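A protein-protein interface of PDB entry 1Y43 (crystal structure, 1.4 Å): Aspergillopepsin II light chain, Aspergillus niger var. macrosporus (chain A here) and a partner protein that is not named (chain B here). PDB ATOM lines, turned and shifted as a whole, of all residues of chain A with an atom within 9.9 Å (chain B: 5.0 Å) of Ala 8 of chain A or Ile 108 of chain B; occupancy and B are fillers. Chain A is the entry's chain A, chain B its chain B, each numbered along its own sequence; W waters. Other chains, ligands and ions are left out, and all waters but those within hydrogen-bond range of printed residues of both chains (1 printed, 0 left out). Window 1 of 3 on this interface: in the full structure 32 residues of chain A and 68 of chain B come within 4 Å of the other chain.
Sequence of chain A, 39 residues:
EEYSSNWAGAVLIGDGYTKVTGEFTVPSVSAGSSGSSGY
OE1 of Glu 1 of chain A sits close to OD2 of Asp 150 of chain B (2.7 Å). The backbone NH (N) of Asp 150 of chain B sits at hydrogen-bond distance from the backbone carbonyl oxygen (O) of Glu 2 of chain A, at 2.9 Å. O of Asp 150 of chain B sits at hydrogen-bond distance from N of Ser 4 of chain A (3.0 Å). O of Ala 8 of chain A lies within hydrogen-bond range of N of Val 109 of chain B (2.9 Å). N of Gly 9 of chain A sits at hydrogen-bond distance from O of Met 149 of chain B. The backbone NH (N) of Ala 10 of chain A lies within hydrogen-bond range of the backbone carbonyl oxygen (O) of Trp 107 of chain B, at 3.1 Å. NE1 of Trp 107 of chain B sits at hydrogen-bond distance from O of Thr 21 of chain A (2.9 Å). The side-chain carboxylate (OE2) of Glu 1 of chain A lies close to the backbone carbonyl oxygen (O) of Thr 161 of chain B (3.3 Å).
OG of Ser 4 of chain A sits close to N of Asn 6 of chain A (3.5 Å). The side-chain hydroxyl (OG) of Ser 4 of chain A sits at hydrogen-bond distance from the backbone NH (N) of Trp 7 of chain A, 2.9 Å away. O of Ser 8 of chain B lies within hydrogen-bond range of N of Glu 110 of chain B (2.8 Å). The backbone carbonyl oxygen (O) of Ile 108 of chain B lies within hydrogen-bond range of the backbone NH (N) of Trp 10 of chain B (2.8 Å). The indole nitrogen (NE1) of Trp 10 of chain B is in hydrogen-bond range of the side-chain carboxylate (OE1) of Glu 110 of chain B, at 3.0 Å. The backbone NH (N) of Ile 151 of chain B is in hydrogen-bond range of the side-chain hydroxyl (OG1) of Thr 159 of chain B (3.0 Å).
Among the printed residues, pairs that only touch across the chains: Glu 2 of chain A with Met 149 of chain B, Tyr 3 of chain A with Asp 150 of chain B, Ser 4 of chain A with Ile 151 of chain B, Ser 5 of chain A with Ile 151 of chain B, Asn 6 of chain A with Val 109 of chain B, Asn 6 of chain A with Glu 110 of chain B, Asn 6 of chain A with Ile 151 of chain B, Trp 7 of chain A with Trp 10 of chain B, Trp 7 of chain A with Ile 108 of chain B, Trp 7 of chain A with Val 109 of chain B, Trp 7 of chain A with Glu 110 of chain B, Trp 7 of chain A with Met 149 of chain B, Trp 7 of chain A with Asp 150 of chain B, Trp 7 of chain A with Ile 151 of chain B, Ala 8 of chain A with Ile 108 of chain B, Ala 8 of chain A with Met 149 of chain B, Ala 8 of chain A with Ile 151 of chain B, Ala 8 of chain A with Thr 159 of chain B, Ala 8 of chain A with Val 170 of chain B, Gly 9 of chain A with Trp 107 of chain B, Gly 9 of chain A with Thr 161 of chain B, Ala 10 of chain A with Glu 106 of chain B, Val 11 of chain A with Glu 106 of chain B, Leu 12 of chain A with Trp 107 of chain B, Val 20 of chain A with Glu 106 of chain B, Val 20 of chain A with Trp 107 of chain B and Phe 24 of chain A with Phe 129 of chain B.
Ala 8 of chain A touches just these residues of chain B: Ile 108 (3.4 Å), Val 109 (2.9 Å), Met 149 (3.2 Å), Ile 151 (3.9 Å), Thr 159 (3.4 Å) and Val 170 (3.97 Å). Gly 22 of chain A touches none of the printed residues of chain B. No residue of chain A comes within 4 Å of Ala 9 of chain B. Of chain A, only Trp 7 (3.6 Å) comes within 4 Å of Trp 10 of chain B. Printed residues of chain A within 4 Å of Glu 106 of chain B: Ala 10 (3.3 Å), Val 11 (3.9 Å) and Val 20 (3.9 Å). Ile 108 of chain B touches two residues of chain A. Printed residues of chain A within 4 Å of Thr 161 of chain B: Glu 1 (3.3 Å) and Gly 9 (3.6 Å). The nearest residue of chain B that does not touch Ala 8 of chain A is Asp 150 of chain B (4.05 Å). The nearest printed residue of chain B that does not touch Tyr 3 of chain A is Ile 151 of chain B (4.4 Å).
Hydrophobic or aromatic side chains of chain A within 4 Å of the printed part of chain B: Tyr 3, Trp 7, Ala 8, Val 11, Leu 12, Val 20 and Phe 24. Of the 15 printed residues of chain B, 13 touch a printed residue of chain A. Hydrophobic or aromatic side chains of chain B within 4 Å of the printed part of chain A: Trp 10, Trp 107, Ile 108, Phe 129, Met 149, Ile 151 and Val 170.
Water W1 bridges the side-chain carboxylate (OE2) of Glu 110 of chain B and the side-chain amide nitrogen (ND2) of Asn 6 of chain A.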
ATOM      1  N   GLU A   1     -10.934  19.270  -2.963  1.00  0.00           N
ATOM      2  CA  GLU A   1      -9.764  20.013  -2.396  1.00  0.00           C
ATOM      3  C   GLU A   1      -9.788  19.964  -0.871  1.00  0.00           C
ATOM      4  O   GLU A   1     -10.791  19.575  -0.263  1.00  0.00           O
ATOM      5  CB  GLU A   1      -9.804  21.491  -2.812  1.00  0.00           C
ATOM      6  CG  GLU A   1      -9.790  21.782  -4.312  1.00  0.00           C
ATOM      7  CD  GLU A   1      -9.725  23.281  -4.616  1.00  0.00           C
ATOM      8  OE1 GLU A   1     -10.183  24.088  -3.762  1.00  0.00           O
ATOM      9  OE2 GLU A   1      -9.205  23.651  -5.705  1.00  0.00           O
ATOM     10  N   GLU A   2      -8.698  20.428  -0.269  1.00  0.00           N
ATOM     11  CA  GLU A   2      -8.546  20.489   1.184  1.00  0.00           C
ATOM     12  C   GLU A   2      -8.223  21.945   1.503  1.00  0.00           C
ATOM     13  O   GLU A   2      -7.463  22.586   0.768  1.00  0.00           O
ATOM     14  CB  GLU A   2      -7.379  19.607   1.631  1.00  0.00           C
ATOM     15  CG  GLU A   2      -7.731  18.144   1.879  1.00  0.00           C
ATOM     16  CD  GLU A   2      -8.137  17.866   3.327  1.00  0.00           C
ATOM     17  OE1 GLU A   2      -7.785  18.673   4.231  1.00  0.00           O
ATOM     18  OE2 GLU A   2      -8.810  16.833   3.568  1.00  0.00           O
ATOM     19  N   TYR A   3      -8.883  22.502   2.523  1.00  0.00           N
ATOM     20  CA  TYR A   3      -8.625  23.880   2.916  1.00  0.00           C
ATOM     21  C   TYR A   3      -7.709  23.918   4.109  1.00  0.00           C
ATOM     22  O   TYR A   3      -7.660  22.961   4.898  1.00  0.00           O
ATOM     23  CB  TYR A   3      -9.918  24.616   3.269  1.00  0.00           C
ATOM     24  CG  TYR A   3     -10.799  24.881   2.074  1.00  0.00           C
ATOM     25  CD1 TYR A   3     -10.516  25.928   1.185  1.00  0.00           C
ATOM     26  CD2 TYR A   3     -11.890  24.054   1.795  1.00  0.00           C
ATOM     27  CE1 TYR A   3     -11.301  26.135   0.050  1.00  0.00           C
ATOM     28  CE2 TYR A   3     -12.673  24.252   0.665  1.00  0.00           C
ATOM     29  CZ  TYR A   3     -12.372  25.289  -0.208  1.00  0.00           C
ATOM     30  OH  TYR A   3     -13.135  25.451  -1.345  1.00  0.00           O
ATOM     31  N   SER A   4      -6.940  24.982   4.198  1.00  0.00           N
ATOM     32  CA  SER A   4      -6.041  25.191   5.322  1.00  0.00           C
ATOM     33  C   SER A   4      -5.978  26.695   5.471  1.00  0.00           C
ATOM     34  O   SER A   4      -6.456  27.444   4.620  1.00  0.00           O
ATOM     35  CB  SER A   4      -4.658  24.570   5.065  1.00  0.00           C
ATOM     36  OG  SER A   4      -3.836  25.401   4.262  1.00  0.00           O
ATOM     37  N   SER A   5      -5.456  27.158   6.605  1.00  0.00           N
ATOM     38  CA  SER A   5      -5.344  28.592   6.849  1.00  0.00           C
ATOM     39  C   SER A   5      -4.117  29.203   6.190  1.00  0.00           C
ATOM     40  O   SER A   5      -4.080  30.412   5.963  1.00  0.00           O
ATOM     41  CB  SER A   5      -5.173  28.853   8.363  1.00  0.00           C
ATOM     42  OG  SER A   5      -6.069  28.086   9.163  1.00  0.00           O
ATOM     43  N   ASN A   6      -3.117  28.366   5.926  1.00  0.00           N
ATOM     44  CA  ASN A   6      -1.839  28.892   5.454  1.00  0.00           C
ATOM     45  C   ASN A   6      -1.229  28.348   4.161  1.00  0.00           C
ATOM     46  O   ASN A   6      -0.374  29.027   3.593  1.00  0.00           O
ATOM     47  CB  ASN A   6      -0.830  28.718   6.569  1.00  0.00           C
ATOM     48  CG  ASN A   6      -0.710  27.277   7.055  1.00  0.00           C
ATOM     49  OD1 ASN A   6      -1.539  26.442   6.713  1.00  0.00           O
ATOM     50  ND2 ASN A   6       0.299  26.999   7.856  1.00  0.00           N
ATOM     51  N   TRP A   7      -1.634  27.171   3.703  1.00  0.00           N
ATOM     52  CA  TRP A   7      -1.070  26.582   2.473  1.00  0.00           C
ATOM     53  C   TRP A   7      -2.046  26.450   1.309  1.00  0.00           C
ATOM     54  O   TRP A   7      -3.157  25.976   1.457  1.00  0.00           O
ATOM     55  CB  TRP A   7      -0.587  25.160   2.722  1.00  0.00           C
ATOM     56  CG  TRP A   7       0.677  24.967   3.491  1.00  0.00           C
ATOM     57  CD1 TRP A   7       1.284  25.862   4.328  1.00  0.00           C
ATOM     58  CD2 TRP A   7       1.473  23.763   3.534  1.00  0.00           C
ATOM     59  NE1 TRP A   7       2.403  25.269   4.884  1.00  0.00           N
ATOM     60  CE2 TRP A   7       2.539  24.001   4.426  1.00  0.00           C
ATOM     61  CE3 TRP A   7       1.373  22.506   2.901  1.00  0.00           C
ATOM     62  CZ2 TRP A   7       3.509  23.016   4.705  1.00  0.00           C
ATOM     63  CZ3 TRP A   7       2.338  21.536   3.177  1.00  0.00           C
ATOM     64  CH2 TRP A   7       3.387  21.800   4.074  1.00  0.00           C
ATOM     65  N   ALA A   8      -1.588  26.770   0.111  1.00  0.00           N
ATOM     66  CA  ALA A   8      -2.398  26.564  -1.094  1.00  0.00           C
ATOM     67  C   ALA A   8      -1.405  25.910  -2.047  1.00  0.00           C
ATOM     68  O   ALA A   8      -0.205  26.212  -1.992  1.00  0.00           O
ATOM     69  CB  ALA A   8      -2.872  27.867  -1.679  1.00  0.00           C
ATOM     70  N   GLY A   9      -1.848  24.959  -2.861  1.00  0.00           N
ATOM     71  CA  GLY A   9      -0.920  24.313  -3.771  1.00  0.00           C
ATOM     72  C   GLY A   9      -1.177  22.825  -3.940  1.00  0.00           C
ATOM     73  O   GLY A   9      -2.311  22.362  -3.785  1.00  0.00           O
ATOM     74  N   ALA A  10      -0.116  22.070  -4.189  1.00  0.00           N
ATOM     75  CA  ALA A  10      -0.223  20.631  -4.415  1.00  0.00           C
ATOM     76  C   ALA A  10       0.755  19.866  -3.542  1.00  0.00           C
ATOM     77  O   ALA A  10       1.938  20.200  -3.505  1.00  0.00           O
ATOM     78  CB  ALA A  10       0.045  20.318  -5.888  1.00  0.00           C
ATOM     79  N   VAL A  11       0.266  18.817  -2.879  1.00  0.00           N
ATOM     80  CA  VAL A  11       1.097  17.988  -2.005  1.00  0.00           C
ATOM     81  C   VAL A  11       0.997  16.503  -2.389  1.00  0.00           C
ATOM     82  O   VAL A  11      -0.107  15.945  -2.460  1.00  0.00           O
ATOM     83  CB  VAL A  11       0.671  18.120  -0.509  1.00  0.00           C
ATOM     84  CG1 VAL A  11       1.660  17.385   0.393  1.00  0.00           C
ATOM     85  CG2 VAL A  11       0.555  19.594  -0.093  1.00  0.00           C
ATOM     86  N   LEU A  12       2.137  15.893  -2.705  1.00  0.00           N
ATOM     87  CA  LEU A  12       2.186  14.468  -3.014  1.00  0.00           C
ATOM     88  C   LEU A  12       2.434  13.746  -1.696  1.00  0.00           C
ATOM     89  O   LEU A  12       3.266  14.177  -0.898  1.00  0.00           O
ATOM     90  CB  LEU A  12       3.335  14.135  -3.969  1.00  0.00           C
ATOM     91  CG  LEU A  12       3.163  14.449  -5.455  1.00  0.00           C
ATOM     92  CD1 LEU A  12       4.483  14.193  -6.150  1.00  0.00           C
ATOM     93  CD2 LEU A  12       2.059  13.594  -6.070  1.00  0.00           C
ATOM     94  N   VAL A  20      12.694  17.704  -5.049  1.00  0.00           N
ATOM     95  CA  VAL A  20      11.477  18.365  -5.519  1.00  0.00           C
ATOM     96  C   VAL A  20      11.951  19.639  -6.196  1.00  0.00           C
ATOM     97  O   VAL A  20      12.799  20.360  -5.658  1.00  0.00           O
ATOM     98  CB  VAL A  20      10.504  18.747  -4.384  1.00  0.00           C
ATOM     99  CG1 VAL A  20       9.226  19.326  -4.982  1.00  0.00           C
ATOM    100  CG2 VAL A  20      10.194  17.545  -3.515  1.00  0.00           C
ATOM    101  N   THR A  21      11.428  19.911  -7.382  1.00  0.00           N
ATOM    102  CA  THR A  21      11.825  21.097  -8.108  1.00  0.00           C
ATOM    103  C   THR A  21      10.629  21.721  -8.827  1.00  0.00           C
ATOM    104  O   THR A  21       9.616  21.056  -9.064  1.00  0.00           O
ATOM    105  CB  THR A  21      12.971  20.776  -9.109  1.00  0.00           C
ATOM    106  OG1 THR A  21      13.417  21.978  -9.736  1.00  0.00           O
ATOM    107  CG2 THR A  21      12.518  19.783 -10.187  1.00  0.00           C
ATOM    108  N   GLY A  22      10.733  23.009  -9.117  1.00  0.00           N
ATOM    109  CA  GLY A  22       9.683  23.715  -9.827  1.00  0.00           C
ATOM    110  C   GLY A  22      10.240  25.017 -10.357  1.00  0.00           C
ATOM    111  O   GLY A  22      11.211  25.550  -9.818  1.00  0.00           O
ATOM    112  N   PHE A  24       8.990  29.016 -11.627  1.00  0.00           N
ATOM    113  CA  PHE A  24       7.893  29.978 -11.676  1.00  0.00           C
ATOM    114  C   PHE A  24       8.389  31.384 -11.992  1.00  0.00           C
ATOM    115  O   PHE A  24       9.565  31.703 -11.845  1.00  0.00           O
ATOM    116  CB  PHE A  24       7.094  29.997 -10.359  1.00  0.00           C
ATOM    117  CG  PHE A  24       7.893  30.445  -9.155  1.00  0.00           C
ATOM    118  CD1 PHE A  24       8.614  29.521  -8.407  1.00  0.00           C
ATOM    119  CD2 PHE A  24       7.918  31.790  -8.767  1.00  0.00           C
ATOM    120  CE1 PHE A  24       9.357  29.917  -7.288  1.00  0.00           C
ATOM    121  CE2 PHE A  24       8.661  32.195  -7.647  1.00  0.00           C
ATOM    122  CZ  PHE A  24       9.376  31.253  -6.912  1.00  0.00           C
ATOM    123  N   SER B   8       4.317  33.862  -0.128  1.00  0.00           N
ATOM    124  CA  SER B   8       5.562  33.177  -0.445  1.00  0.00           C
ATOM    125  C   SER B   8       5.251  31.995  -1.373  1.00  0.00           C
ATOM    126  O   SER B   8       4.129  31.469  -1.373  1.00  0.00           O
ATOM    127  CB  SER B   8       6.233  32.672   0.839  1.00  0.00           C
ATOM    128  OG  SER B   8       5.476  31.617   1.416  1.00  0.00           O
ATOM    129  N   ALA B   9       6.235  31.588  -2.158  1.00  0.00           N
ATOM    130  CA  ALA B   9       6.083  30.439  -3.041  1.00  0.00           C
ATOM    131  C   ALA B   9       7.336  29.615  -2.789  1.00  0.00           C
ATOM    132  O   ALA B   9       8.453  30.149  -2.795  1.00  0.00           O
ATOM    133  CB  ALA B   9       6.032  30.872  -4.498  1.00  0.00           C
ATOM    134  N   TRP B  10       7.161  28.319  -2.580  1.00  0.00           N
ATOM    135  CA  TRP B  10       8.293  27.451  -2.309  1.00  0.00           C
ATOM    136  C   TRP B  10       8.028  25.994  -2.677  1.00  0.00           C
ATOM    137  O   TRP B  10       6.896  25.616  -2.964  1.00  0.00           O
ATOM    138  CB  TRP B  10       8.648  27.542  -0.811  1.00  0.00           C
ATOM    139  CG  TRP B  10       7.498  27.324   0.131  1.00  0.00           C
ATOM    140  CD1 TRP B  10       6.656  28.280   0.641  1.00  0.00           C
ATOM    141  CD2 TRP B  10       7.103  26.083   0.735  1.00  0.00           C
ATOM    142  NE1 TRP B  10       5.779  27.711   1.528  1.00  0.00           N
ATOM    143  CE2 TRP B  10       6.030  26.365   1.605  1.00  0.00           C
ATOM    144  CE3 TRP B  10       7.560  24.762   0.627  1.00  0.00           C
ATOM    145  CZ2 TRP B  10       5.404  25.372   2.372  1.00  0.00           C
ATOM    146  CZ3 TRP B  10       6.932  23.773   1.394  1.00  0.00           C
ATOM    147  CH2 TRP B  10       5.868  24.087   2.253  1.00  0.00           C
ATOM    148  N   GLU B 106       6.005  18.890  -2.121  1.00  0.00           N
ATOM    149  CA  GLU B 106       4.988  19.911  -2.400  1.00  0.00           C
ATOM    150  C   GLU B 106       5.467  21.175  -3.095  1.00  0.00           C
ATOM    151  O   GLU B 106       6.653  21.491  -3.069  1.00  0.00           O
ATOM    152  CB  GLU B 106       4.264  20.279  -1.088  1.00  0.00           C
ATOM    153  CG  GLU B 106       5.151  20.910  -0.009  1.00  0.00           C
ATOM    154  CD  GLU B 106       5.692  19.926   1.033  1.00  0.00           C
ATOM    155  OE1 GLU B 106       5.231  18.773   1.108  1.00  0.00           O
ATOM    156  OE2 GLU B 106       6.614  20.321   1.774  1.00  0.00           O
ATOM    157  N   TRP B 107       4.507  21.852  -3.744  1.00  0.00           N
ATOM    158  CA  TRP B 107       4.684  23.112  -4.472  1.00  0.00           C
ATOM    159  C   TRP B 107       3.624  23.981  -3.806  1.00  0.00           C
ATOM    160  O   TRP B 107       2.421  23.766  -4.008  1.00  0.00           O
ATOM    161  CB  TRP B 107       4.377  22.912  -5.960  1.00  0.00           C
ATOM    162  CG  TRP B 107       5.295  21.915  -6.620  1.00  0.00           C
ATOM    163  CD1 TRP B 107       6.484  22.180  -7.235  1.00  0.00           C
ATOM    164  CD2 TRP B 107       5.104  20.491  -6.686  1.00  0.00           C
ATOM    165  NE1 TRP B 107       7.046  20.994  -7.675  1.00  0.00           N
ATOM    166  CE2 TRP B 107       6.228  19.957  -7.360  1.00  0.00           C
ATOM    167  CE3 TRP B 107       4.094  19.626  -6.242  1.00  0.00           C
ATOM    168  CZ2 TRP B 107       6.368  18.574  -7.592  1.00  0.00           C
ATOM    169  CZ3 TRP B 107       4.238  18.255  -6.475  1.00  0.00           C
ATOM    170  CH2 TRP B 107       5.369  17.748  -7.145  1.00  0.00           C
ATOM    171  N   ILE B 108       4.064  24.981  -3.042  1.00  0.00           N
ATOM    172  CA  ILE B 108       3.144  25.777  -2.232  1.00  0.00           C
ATOM    173  C   ILE B 108       3.277  27.301  -2.283  1.00  0.00           C
ATOM    174  O   ILE B 108       4.365  27.829  -2.480  1.00  0.00           O
ATOM    175  CB  ILE B 108       3.361  25.368  -0.722  1.00  0.00           C
ATOM    176  CG1 ILE B 108       3.114  23.863  -0.511  1.00  0.00           C
ATOM    177  CG2 ILE B 108       2.507  26.205   0.228  1.00  0.00           C
ATOM    178  CD1 ILE B 108       1.657  23.429  -0.654  1.00  0.00           C
ATOM    179  N   VAL B 109       2.122  27.974  -2.188  1.00  0.00           N
ATOM    180  CA  VAL B 109       2.050  29.424  -2.054  1.00  0.00           C
ATOM    181  C   VAL B 109       1.468  29.540  -0.631  1.00  0.00           C
ATOM    182  O   VAL B 109       0.396  29.001  -0.324  1.00  0.00           O
ATOM    183  CB  VAL B 109       1.138  30.099  -3.099  1.00  0.00           C
ATOM    184  CG1 VAL B 109       0.963  31.568  -2.756  1.00  0.00           C
ATOM    185  CG2 VAL B 109       1.757  29.984  -4.488  1.00  0.00           C
ATOM    186  N   GLU B 110       2.191  30.219   0.244  1.00  0.00           N
ATOM    187  CA  GLU B 110       1.796  30.309   1.639  1.00  0.00           C
ATOM    188  C   GLU B 110       1.579  31.695   2.216  1.00  0.00           C
ATOM    189  O   GLU B 110       2.194  32.677   1.780  1.00  0.00           O
ATOM    190  CB  GLU B 110       2.861  29.596   2.482  1.00  0.00           C
ATOM    191  CG  GLU B 110       2.683  29.725   3.990  1.00  0.00           C
ATOM    192  CD  GLU B 110       3.750  28.994   4.798  1.00  0.00           C
ATOM    193  OE1 GLU B 110       4.606  28.297   4.224  1.00  0.00           O
ATOM    194  OE2 GLU B 110       3.723  29.119   6.032  1.00  0.00           O
ATOM    195  N   PHE B 129       3.759  26.965 -11.201  1.00  0.00           N
ATOM    196  CA  PHE B 129       4.998  26.208 -11.113  1.00  0.00           C
ATOM    197  C   PHE B 129       4.997  25.304 -12.348  1.00  0.00           C
ATOM    198  O   PHE B 129       4.045  24.545 -12.552  1.00  0.00           O
ATOM    199  CB  PHE B 129       4.994  25.291  -9.892  1.00  0.00           C
ATOM    200  CG  PHE B 129       5.078  26.007  -8.568  1.00  0.00           C
ATOM    201  CD1 PHE B 129       3.923  26.378  -7.880  1.00  0.00           C
ATOM    202  CD2 PHE B 129       6.312  26.231  -7.973  1.00  0.00           C
ATOM    203  CE1 PHE B 129       4.004  26.956  -6.595  1.00  0.00           C
ATOM    204  CE2 PHE B 129       6.397  26.805  -6.695  1.00  0.00           C
ATOM    205  CZ  PHE B 129       5.247  27.164  -6.013  1.00  0.00           C
ATOM    206  N   MET B 149      -4.697  21.802  -2.242  1.00  0.00           N
ATOM    207  CA  MET B 149      -5.023  22.604  -1.071  1.00  0.00           C
ATOM    208  C   MET B 149      -5.247  24.065  -1.421  1.00  0.00           C
ATOM    209  O   MET B 149      -4.627  24.590  -2.349  1.00  0.00           O
ATOM    210  CB  MET B 149      -3.892  22.540  -0.036  1.00  0.00           C
ATOM    211  CG  MET B 149      -3.814  21.245   0.747  1.00  0.00           C
ATOM    212  SD  MET B 149      -2.574  21.415   2.026  1.00  0.00           S
ATOM    213  CE  MET B 149      -2.491  19.734   2.603  1.00  0.00           C
ATOM    214  N   ASP B 150      -6.159  24.706  -0.691  1.00  0.00           N
ATOM    215  CA  ASP B 150      -6.435  26.125  -0.869  1.00  0.00           C
ATOM    216  C   ASP B 150      -6.612  26.792   0.477  1.00  0.00           C
ATOM    217  O   ASP B 150      -6.942  26.139   1.461  1.00  0.00           O
ATOM    218  CB  ASP B 150      -7.649  26.369  -1.760  1.00  0.00           C
ATOM    219  CG  ASP B 150      -7.305  26.306  -3.224  1.00  0.00           C
ATOM    220  OD1 ASP B 150      -6.419  27.045  -3.684  1.00  0.00           O
ATOM    221  OD2 ASP B 150      -7.895  25.482  -3.918  1.00  0.00           O
ATOM    222  N   ILE B 151      -6.374  28.098   0.503  1.00  0.00           N
ATOM    223  CA  ILE B 151      -6.472  28.884   1.722  1.00  0.00           C
ATOM    224  C   ILE B 151      -7.885  29.423   1.974  1.00  0.00           C
ATOM    225  O   ILE B 151      -8.543  29.966   1.076  1.00  0.00           O
ATOM    226  CB  ILE B 151      -5.455  30.063   1.716  1.00  0.00           C
ATOM    227  CG1 ILE B 151      -4.027  29.524   1.690  1.00  0.00           C
ATOM    228  CG2 ILE B 151      -5.658  30.966   2.935  1.00  0.00           C
ATOM    229  CD1 ILE B 151      -2.955  30.591   1.487  1.00  0.00           C
ATOM    230  N   THR B 159      -7.822  31.458  -2.368  1.00  0.00           N
ATOM    231  CA  THR B 159      -7.106  30.892  -3.510  1.00  0.00           C
ATOM    232  C   THR B 159      -7.891  29.783  -4.197  1.00  0.00           C
ATOM    233  O   THR B 159      -8.797  29.179  -3.606  1.00  0.00           O
ATOM    234  CB  THR B 159      -5.723  30.264  -3.103  1.00  0.00           C
ATOM    235  OG1 THR B 159      -5.929  29.157  -2.215  1.00  0.00           O
ATOM    236  CG2 THR B 159      -4.827  31.286  -2.421  1.00  0.00           C
ATOM    237  N   THR B 161      -6.708  26.507  -6.720  1.00  0.00           N
ATOM    238  CA  THR B 161      -5.567  25.792  -7.253  1.00  0.00           C
ATOM    239  C   THR B 161      -5.976  24.747  -8.279  1.00  0.00           C
ATOM    240  O   THR B 161      -7.006  24.091  -8.130  1.00  0.00           O
ATOM    241  CB  THR B 161      -4.787  25.112  -6.093  1.00  0.00           C
ATOM    242  OG1 THR B 161      -4.240  26.122  -5.237  1.00  0.00           O
ATOM    243  CG2 THR B 161      -3.660  24.234  -6.616  1.00  0.00           C
ATOM    244  N   VAL B 170      -1.708  28.425  -8.820  1.00  0.00           N
ATOM    245  CA  VAL B 170      -2.432  28.951  -7.668  1.00  0.00           C
ATOM    246  C   VAL B 170      -2.862  30.359  -8.040  1.00  0.00           C
ATOM    247  O   VAL B 170      -2.027  31.200  -8.384  1.00  0.00           O
ATOM    248  CB  VAL B 170      -1.543  29.030  -6.387  1.00  0.00           C
ATOM    249  CG1 VAL B 170      -2.350  29.590  -5.212  1.00  0.00           C
ATOM    250  CG2 VAL B 170      -0.977  27.665  -6.046  1.00  0.00           C
HETATM  251  O   HOH W   1       1.745  29.947   8.372  1.00  0.00           O
